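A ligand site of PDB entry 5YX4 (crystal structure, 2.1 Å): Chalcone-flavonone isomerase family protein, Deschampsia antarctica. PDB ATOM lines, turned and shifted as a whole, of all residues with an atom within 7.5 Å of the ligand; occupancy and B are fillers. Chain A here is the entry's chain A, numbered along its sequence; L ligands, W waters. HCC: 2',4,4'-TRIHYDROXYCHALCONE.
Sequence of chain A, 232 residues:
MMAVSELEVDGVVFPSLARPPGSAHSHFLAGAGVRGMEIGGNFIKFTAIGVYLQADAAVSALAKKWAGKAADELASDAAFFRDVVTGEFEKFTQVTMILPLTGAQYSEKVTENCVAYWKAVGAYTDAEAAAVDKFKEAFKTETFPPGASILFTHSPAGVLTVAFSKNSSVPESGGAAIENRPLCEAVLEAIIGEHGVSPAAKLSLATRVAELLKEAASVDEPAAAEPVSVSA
NE of Arg 35 is in hydrogen-bond range of O19 of the ligand.
O10 of the ligand sits at hydrogen-bond distance from O of Gln 105 (3.4 Å).
N of Leu 99 is in hydrogen-bond range of O of Phe 46 (3.1 Å).
The backbone NH of Arg 35 lies within hydrogen-bond range of the backbone carbonyl oxygen of Thr 47 (2.8 Å).
The backbone carbonyl oxygen (O) of Arg 35 lies within hydrogen-bond range of the backbone NH (N) of Phe 46.
The backbone NH of Thr 102 is in hydrogen-bond range of the side-chain amide oxygen of Gln 105 (3.0 Å).
Residues that only touch the ligand: Lys 109, Tyr 106, Phe 46 and Leu 101.
Within 4 Å of the ligand: Arg 35, Phe 46, Leu 101, Gln 105, Tyr 106 and Lys 109.
The nearest printed residue that does not touch the ligand is Met 37 (4.2 Å).
Water W3 bridges OG1 of Thr 47 (2.6 Å) and O19 of the ligand (2.7 Å).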
ATOM      1  N   ARG A  35     -23.659 -20.143  -7.234  1.00  0.00           N
ATOM      2  CA  ARG A  35     -23.760 -18.851  -6.570  1.00  0.00           C
ATOM      3  C   ARG A  35     -22.611 -18.718  -5.551  1.00  0.00           C
ATOM      4  O   ARG A  35     -22.482 -19.531  -4.634  1.00  0.00           O
ATOM      5  CB  ARG A  35     -25.093 -18.705  -5.908  1.00  0.00           C
ATOM      6  CG  ARG A  35     -25.331 -17.383  -5.184  1.00  0.00           C
ATOM      7  CD  ARG A  35     -24.679 -17.216  -3.805  1.00  0.00           C
ATOM      8  NE  ARG A  35     -25.329 -16.172  -3.015  1.00  0.00           N
ATOM      9  CZ  ARG A  35     -24.956 -14.901  -3.003  1.00  0.00           C
ATOM     10  NH1 ARG A  35     -23.913 -14.456  -3.671  1.00  0.00           N
ATOM     11  NH2 ARG A  35     -25.598 -14.093  -2.257  1.00  0.00           N
ATOM     12  N   GLY A  36     -21.843 -17.671  -5.692  1.00  0.00           N
ATOM     13  CA  GLY A  36     -20.730 -17.426  -4.886  1.00  0.00           C
ATOM     14  C   GLY A  36     -20.548 -15.975  -4.499  1.00  0.00           C
ATOM     15  O   GLY A  36     -21.445 -15.112  -4.709  1.00  0.00           O
ATOM     16  N   MET A  37     -19.391 -15.736  -3.838  1.00  0.00           N
ATOM     17  CA  MET A  37     -18.985 -14.361  -3.389  1.00  0.00           C
ATOM     18  C   MET A  37     -17.500 -14.296  -3.584  1.00  0.00           C
ATOM     19  O   MET A  37     -16.781 -15.320  -3.410  1.00  0.00           O
ATOM     20  CB  MET A  37     -19.363 -14.092  -1.946  1.00  0.00           C
ATOM     21  CG  MET A  37     -20.726 -14.580  -1.576  1.00  0.00           C
ATOM     22  SD  MET A  37     -21.338 -14.247   0.076  1.00  0.00           S
ATOM     23  CE  MET A  37     -21.512 -12.488   0.148  1.00  0.00           C
ATOM     24  N   ILE A  39     -14.038 -13.024  -2.186  1.00  0.00           N
ATOM     25  CA  ILE A  39     -13.648 -12.704  -0.784  1.00  0.00           C
ATOM     26  C   ILE A  39     -12.210 -12.927  -0.810  1.00  0.00           C
ATOM     27  O   ILE A  39     -11.769 -14.036  -1.007  1.00  0.00           O
ATOM     28  CB  ILE A  39     -14.253 -13.614   0.287  1.00  0.00           C
ATOM     29  CG1 ILE A  39     -15.749 -13.802   0.058  1.00  0.00           C
ATOM     30  CG2 ILE A  39     -13.946 -13.057   1.672  1.00  0.00           C
ATOM     31  CD1 ILE A  39     -16.422 -14.865   0.913  1.00  0.00           C
ATOM     32  N   ILE A  44     -15.631 -17.887  -3.724  1.00  0.00           N
ATOM     33  CA  ILE A  44     -16.071 -18.822  -2.766  1.00  0.00           C
ATOM     34  C   ILE A  44     -17.511 -19.267  -3.147  1.00  0.00           C
ATOM     35  O   ILE A  44     -18.438 -18.491  -3.013  1.00  0.00           O
ATOM     36  CB  ILE A  44     -16.069 -18.152  -1.337  1.00  0.00           C
ATOM     37  CG1 ILE A  44     -14.654 -17.578  -0.956  1.00  0.00           C
ATOM     38  CG2 ILE A  44     -16.564 -19.157  -0.276  1.00  0.00           C
ATOM     39  CD1 ILE A  44     -13.506 -18.523  -1.242  1.00  0.00           C
ATOM     40  N   PHE A  46     -21.050 -20.828  -2.578  1.00  0.00           N
ATOM     41  CA  PHE A  46     -21.970 -21.038  -1.499  1.00  0.00           C
ATOM     42  C   PHE A  46     -23.118 -22.002  -1.779  1.00  0.00           C
ATOM     43  O   PHE A  46     -23.492 -22.818  -0.895  1.00  0.00           O
ATOM     44  CB  PHE A  46     -22.531 -19.765  -1.061  1.00  0.00           C
ATOM     45  CG  PHE A  46     -21.671 -19.050  -0.077  1.00  0.00           C
ATOM     46  CD1 PHE A  46     -20.585 -18.319  -0.510  1.00  0.00           C
ATOM     47  CD2 PHE A  46     -21.940 -19.140   1.278  1.00  0.00           C
ATOM     48  CE1 PHE A  46     -19.782 -17.642   0.393  1.00  0.00           C
ATOM     49  CE2 PHE A  46     -21.133 -18.496   2.199  1.00  0.00           C
ATOM     50  CZ  PHE A  46     -20.056 -17.761   1.765  1.00  0.00           C
ATOM     51  N   THR A  47     -23.716 -21.869  -2.979  1.00  0.00           N
ATOM     52  CA  THR A  47     -24.940 -22.621  -3.351  1.00  0.00           C
ATOM     53  C   THR A  47     -24.882 -22.980  -4.842  1.00  0.00           C
ATOM     54  O   THR A  47     -24.024 -22.429  -5.603  1.00  0.00           O
ATOM     55  CB  THR A  47     -26.268 -21.915  -3.009  1.00  0.00           C
ATOM     56  OG1 THR A  47     -26.444 -20.694  -3.759  1.00  0.00           O
ATOM     57  CG2 THR A  47     -26.390 -21.641  -1.525  1.00  0.00           C
ATOM     58  N   ILE A  49     -27.722 -23.299  -7.890  1.00  0.00           N
ATOM     59  CA  ILE A  49     -29.116 -22.855  -8.119  1.00  0.00           C
ATOM     60  C   ILE A  49     -29.603 -23.391  -9.513  1.00  0.00           C
ATOM     61  O   ILE A  49     -28.900 -23.241 -10.506  1.00  0.00           O
ATOM     62  CB  ILE A  49     -29.245 -21.324  -8.072  1.00  0.00           C
ATOM     63  CG1 ILE A  49     -28.794 -20.816  -6.679  1.00  0.00           C
ATOM     64  CG2 ILE A  49     -30.696 -20.917  -8.248  1.00  0.00           C
ATOM     65  CD1 ILE A  49     -28.771 -19.318  -6.506  1.00  0.00           C
ATOM     66  N   VAL A  95     -32.502 -24.040  -4.583  1.00  0.00           N
ATOM     67  CA  VAL A  95     -31.213 -23.584  -4.065  1.00  0.00           C
ATOM     68  C   VAL A  95     -30.611 -24.692  -3.194  1.00  0.00           C
ATOM     69  O   VAL A  95     -31.138 -24.994  -2.127  1.00  0.00           O
ATOM     70  CB  VAL A  95     -31.407 -22.347  -3.187  1.00  0.00           C
ATOM     71  CG1 VAL A  95     -30.050 -21.862  -2.648  1.00  0.00           C
ATOM     72  CG2 VAL A  95     -32.113 -21.245  -3.939  1.00  0.00           C
ATOM     73  N   MET A  97     -27.410 -26.135  -1.061  1.00  0.00           N
ATOM     74  CA  MET A  97     -26.155 -25.750  -0.317  1.00  0.00           C
ATOM     75  C   MET A  97     -24.896 -26.441  -0.692  1.00  0.00           C
ATOM     76  O   MET A  97     -24.814 -27.667  -0.773  1.00  0.00           O
ATOM     77  CB  MET A  97     -26.301 -26.017   1.182  1.00  0.00           C
ATOM     78  CG  MET A  97     -27.452 -25.325   1.853  1.00  0.00           C
ATOM     79  SD  MET A  97     -27.715 -23.631   1.305  1.00  0.00           S
ATOM     80  CE  MET A  97     -29.427 -23.629   0.932  1.00  0.00           C
ATOM     81  N   LEU A  99     -21.867 -24.774   0.858  1.00  0.00           N
ATOM     82  CA  LEU A  99     -21.496 -24.498   2.230  1.00  0.00           C
ATOM     83  C   LEU A  99     -22.752 -24.463   3.052  1.00  0.00           C
ATOM     84  O   LEU A  99     -23.828 -24.157   2.507  1.00  0.00           O
ATOM     85  CB  LEU A  99     -20.819 -23.161   2.339  1.00  0.00           C
ATOM     86  CG  LEU A  99     -19.420 -23.094   1.734  1.00  0.00           C
ATOM     87  CD1 LEU A  99     -18.843 -21.699   1.903  1.00  0.00           C
ATOM     88  CD2 LEU A  99     -18.442 -24.134   2.295  1.00  0.00           C
ATOM     89  N   PRO A 100     -22.626 -24.710   4.381  1.00  0.00           N
ATOM     90  CA  PRO A 100     -23.829 -24.705   5.198  1.00  0.00           C
ATOM     91  C   PRO A 100     -24.400 -23.348   5.460  1.00  0.00           C
ATOM     92  O   PRO A 100     -23.659 -22.392   5.612  1.00  0.00           O
ATOM     93  CB  PRO A 100     -23.408 -25.441   6.528  1.00  0.00           C
ATOM     94  CG  PRO A 100     -21.959 -25.646   6.466  1.00  0.00           C
ATOM     95  CD  PRO A 100     -21.494 -25.446   5.035  1.00  0.00           C
ATOM     96  N   LEU A 101     -25.721 -23.240   5.543  1.00  0.00           N
ATOM     97  CA  LEU A 101     -26.310 -22.007   5.951  1.00  0.00           C
ATOM     98  C   LEU A 101     -27.496 -22.290   6.851  1.00  0.00           C
ATOM     99  O   LEU A 101     -28.139 -23.335   6.729  1.00  0.00           O
ATOM    100  CB  LEU A 101     -26.858 -21.282   4.721  1.00  0.00           C
ATOM    101  CG  LEU A 101     -25.918 -20.813   3.606  1.00  0.00           C
ATOM    102  CD1 LEU A 101     -26.757 -20.262   2.411  1.00  0.00           C
ATOM    103  CD2 LEU A 101     -24.984 -19.717   4.128  1.00  0.00           C
ATOM    104  N   THR A 102     -27.828 -21.358   7.709  1.00  0.00           N
ATOM    105  CA  THR A 102     -28.943 -21.463   8.551  1.00  0.00           C
ATOM    106  C   THR A 102     -30.119 -20.723   7.909  1.00  0.00           C
ATOM    107  O   THR A 102     -29.939 -19.793   7.075  1.00  0.00           O
ATOM    108  CB  THR A 102     -28.670 -20.861   9.947  1.00  0.00           C
ATOM    109  OG1 THR A 102     -28.558 -19.457   9.862  1.00  0.00           O
ATOM    110  CG2 THR A 102     -27.367 -21.436  10.584  1.00  0.00           C
ATOM    111  N   GLY A 103     -31.299 -21.101   8.348  1.00  0.00           N
ATOM    112  CA  GLY A 103     -32.539 -20.460   7.991  1.00  0.00           C
ATOM    113  C   GLY A 103     -32.554 -18.981   8.232  1.00  0.00           C
ATOM    114  O   GLY A 103     -33.034 -18.188   7.375  1.00  0.00           O
ATOM    115  N   ALA A 104     -32.045 -18.576   9.402  1.00  0.00           N
ATOM    116  CA  ALA A 104     -32.050 -17.174   9.848  1.00  0.00           C
ATOM    117  C   ALA A 104     -31.086 -16.388   8.962  1.00  0.00           C
ATOM    118  O   ALA A 104     -31.469 -15.324   8.517  1.00  0.00           O
ATOM    119  CB  ALA A 104     -31.698 -17.002  11.351  1.00  0.00           C
ATOM    120  N   GLN A 105     -29.870 -16.920   8.702  1.00  0.00           N
ATOM    121  CA  GLN A 105     -28.928 -16.302   7.756  1.00  0.00           C
ATOM    122  C   GLN A 105     -29.593 -16.045   6.372  1.00  0.00           C
ATOM    123  O   GLN A 105     -29.666 -14.915   5.951  1.00  0.00           O
ATOM    124  CB  GLN A 105     -27.716 -17.157   7.497  1.00  0.00           C
ATOM    125  CG  GLN A 105     -26.677 -17.186   8.603  1.00  0.00           C
ATOM    126  CD  GLN A 105     -25.492 -18.056   8.194  1.00  0.00           C
ATOM    127  OE1 GLN A 105     -25.674 -19.231   7.840  1.00  0.00           O
ATOM    128  NE2 GLN A 105     -24.276 -17.495   8.234  1.00  0.00           N
ATOM    129  N   TYR A 106     -30.119 -17.086   5.727  1.00  0.00           N
ATOM    130  CA  TYR A 106     -30.676 -16.964   4.394  1.00  0.00           C
ATOM    131  C   TYR A 106     -31.814 -15.979   4.421  1.00  0.00           C
ATOM    132  O   TYR A 106     -31.788 -15.027   3.670  1.00  0.00           O
ATOM    133  CB  TYR A 106     -31.079 -18.353   3.814  1.00  0.00           C
ATOM    134  CG  TYR A 106     -31.485 -18.330   2.367  1.00  0.00           C
ATOM    135  CD1 TYR A 106     -32.791 -17.983   1.995  1.00  0.00           C
ATOM    136  CD2 TYR A 106     -30.554 -18.556   1.368  1.00  0.00           C
ATOM    137  CE1 TYR A 106     -33.153 -17.901   0.634  1.00  0.00           C
ATOM    138  CE2 TYR A 106     -30.898 -18.505   0.015  1.00  0.00           C
ATOM    139  CZ  TYR A 106     -32.204 -18.179  -0.352  1.00  0.00           C
ATOM    140  OH  TYR A 106     -32.522 -18.098  -1.714  1.00  0.00           O
ATOM    141  N   SER A 107     -32.784 -16.145   5.315  1.00  0.00           N
ATOM    142  CA  SER A 107     -33.970 -15.310   5.299  1.00  0.00           C
ATOM    143  C   SER A 107     -33.732 -13.805   5.607  1.00  0.00           C
ATOM    144  O   SER A 107     -34.416 -12.891   5.057  1.00  0.00           O
ATOM    145  CB  SER A 107     -35.055 -15.857   6.232  1.00  0.00           C
ATOM    146  OG  SER A 107     -34.687 -15.817   7.583  1.00  0.00           O
ATOM    147  N   GLU A 108     -32.803 -13.567   6.546  1.00  0.00           N
ATOM    148  CA  GLU A 108     -32.347 -12.230   6.869  1.00  0.00           C
ATOM    149  C   GLU A 108     -31.651 -11.592   5.657  1.00  0.00           C
ATOM    150  O   GLU A 108     -31.989 -10.461   5.328  1.00  0.00           O
ATOM    151  CB  GLU A 108     -31.438 -12.201   8.109  1.00  0.00           C
ATOM    152  CG  GLU A 108     -32.237 -12.356   9.407  1.00  0.00           C
ATOM    153  CD  GLU A 108     -31.382 -12.496  10.692  1.00  0.00           C
ATOM    154  OE1 GLU A 108     -30.182 -12.111  10.695  1.00  0.00           O
ATOM    155  OE2 GLU A 108     -31.922 -13.016  11.702  1.00  0.00           O
ATOM    156  N   LYS A 109     -30.777 -12.319   5.006  1.00  0.00           N
ATOM    157  CA  LYS A 109     -30.133 -11.750   3.866  1.00  0.00           C
ATOM    158  C   LYS A 109     -31.118 -11.404   2.791  1.00  0.00           C
ATOM    159  O   LYS A 109     -31.091 -10.313   2.294  1.00  0.00           O
ATOM    160  CB  LYS A 109     -29.084 -12.674   3.300  1.00  0.00           C
ATOM    161  CG  LYS A 109     -28.168 -11.951   2.349  1.00  0.00           C
ATOM    162  CD  LYS A 109     -27.397 -12.883   1.475  1.00  0.00           C
ATOM    163  CE  LYS A 109     -25.932 -12.873   1.801  1.00  0.00           C
ATOM    164  NZ  LYS A 109     -25.511 -11.550   2.305  1.00  0.00           N
ATOM    165  N   VAL A 110     -32.013 -12.301   2.433  1.00  0.00           N
ATOM    166  CA  VAL A 110     -32.913 -11.967   1.347  1.00  0.00           C
ATOM    167  C   VAL A 110     -33.923 -10.913   1.703  1.00  0.00           C
ATOM    168  O   VAL A 110     -34.115 -10.028   0.884  1.00  0.00           O
ATOM    169  CB  VAL A 110     -33.539 -13.122   0.437  1.00  0.00           C
ATOM    170  CG1 VAL A 110     -32.900 -14.466   0.603  1.00  0.00           C
ATOM    171  CG2 VAL A 110     -35.066 -13.135   0.403  1.00  0.00           C
ATOM    172  N   ILE A 150     -33.412 -25.464  -0.509  1.00  0.00           N
ATOM    173  CA  ILE A 150     -34.527 -24.622  -0.405  1.00  0.00           C
ATOM    174  C   ILE A 150     -35.301 -24.622  -1.751  1.00  0.00           C
ATOM    175  O   ILE A 150     -34.712 -24.464  -2.804  1.00  0.00           O
ATOM    176  CB  ILE A 150     -34.101 -23.188  -0.085  1.00  0.00           C
ATOM    177  CG1 ILE A 150     -33.231 -23.126   1.159  1.00  0.00           C
ATOM    178  CG2 ILE A 150     -35.344 -22.350   0.055  1.00  0.00           C
ATOM    179  CD1 ILE A 150     -32.366 -21.880   1.170  1.00  0.00           C
ATOM    180  N   ILE A 191     -31.805 -13.559  -7.829  1.00  0.00           N
ATOM    181  CA  ILE A 191     -30.912 -14.497  -8.489  1.00  0.00           C
ATOM    182  C   ILE A 191     -30.527 -14.168  -9.940  1.00  0.00           C
ATOM    183  O   ILE A 191     -29.367 -14.289 -10.292  1.00  0.00           O
ATOM    184  CB  ILE A 191     -31.521 -15.933  -8.409  1.00  0.00           C
ATOM    185  CG1 ILE A 191     -31.699 -16.289  -6.917  1.00  0.00           C
ATOM    186  CG2 ILE A 191     -30.623 -16.930  -9.064  1.00  0.00           C
ATOM    187  CD1 ILE A 191     -32.460 -17.562  -6.615  1.00  0.00           C
ATOM    188  N   VAL A 197     -27.552 -12.534  -7.977  1.00  0.00           N
ATOM    189  CA  VAL A 197     -26.333 -13.139  -7.319  1.00  0.00           C
ATOM    190  C   VAL A 197     -25.781 -14.330  -8.067  1.00  0.00           C
ATOM    191  O   VAL A 197     -24.698 -14.821  -7.753  1.00  0.00           O
ATOM    192  CB  VAL A 197     -26.592 -13.482  -5.848  1.00  0.00           C
ATOM    193  CG1 VAL A 197     -26.994 -12.228  -5.049  1.00  0.00           C
ATOM    194  CG2 VAL A 197     -27.678 -14.534  -5.694  1.00  0.00           C
HETATM  195  C1  HCC L   1     -26.755 -16.830  -0.048  1.00  0.00           C
HETATM  196  C2  HCC L   1     -25.404 -17.071   0.161  1.00  0.00           C
HETATM  197  C3  HCC L   1     -24.814 -16.853   1.396  1.00  0.00           C
HETATM  198  C4  HCC L   1     -25.571 -16.422   2.459  1.00  0.00           C
HETATM  199  C5  HCC L   1     -27.043 -16.161   2.219  1.00  0.00           C
HETATM  200  C6  HCC L   1     -27.589 -16.384   0.963  1.00  0.00           C
HETATM  201  C7  HCC L   1     -24.971 -16.115   3.826  1.00  0.00           C
HETATM  202  C8  HCC L   1     -23.480 -15.935   3.932  1.00  0.00           C
HETATM  203  C9  HCC L   1     -22.923 -15.406   5.016  1.00  0.00           C
HETATM  204  O10 HCC L   1     -27.837 -15.680   3.219  1.00  0.00           O
HETATM  205  C11 HCC L   1     -21.462 -15.259   5.153  1.00  0.00           C
HETATM  206  C12 HCC L   1     -20.594 -15.175   4.067  1.00  0.00           C
HETATM  207  C13 HCC L   1     -19.230 -15.117   4.292  1.00  0.00           C
HETATM  208  C14 HCC L   1     -18.716 -15.174   5.609  1.00  0.00           C
HETATM  209  C15 HCC L   1     -19.568 -15.315   6.689  1.00  0.00           C
HETATM  210  C16 HCC L   1     -20.946 -15.356   6.460  1.00  0.00           C
HETATM  211  O17 HCC L   1     -25.728 -15.799   4.764  1.00  0.00           O
HETATM  212  O18 HCC L   1     -17.385 -15.123   5.786  1.00  0.00           O
HETATM  213  O19 HCC L   1     -27.259 -16.989  -1.290  1.00  0.00           O
HETATM  214  O   HOH W   1     -25.394 -13.851   6.319  1.00  0.00           O
HETATM  215  O   HOH W   2     -29.552 -15.105  -2.123  1.00  0.00           O
HETATM  216  O   HOH W   3     -28.104 -18.853  -3.044  1.00  0.00           O
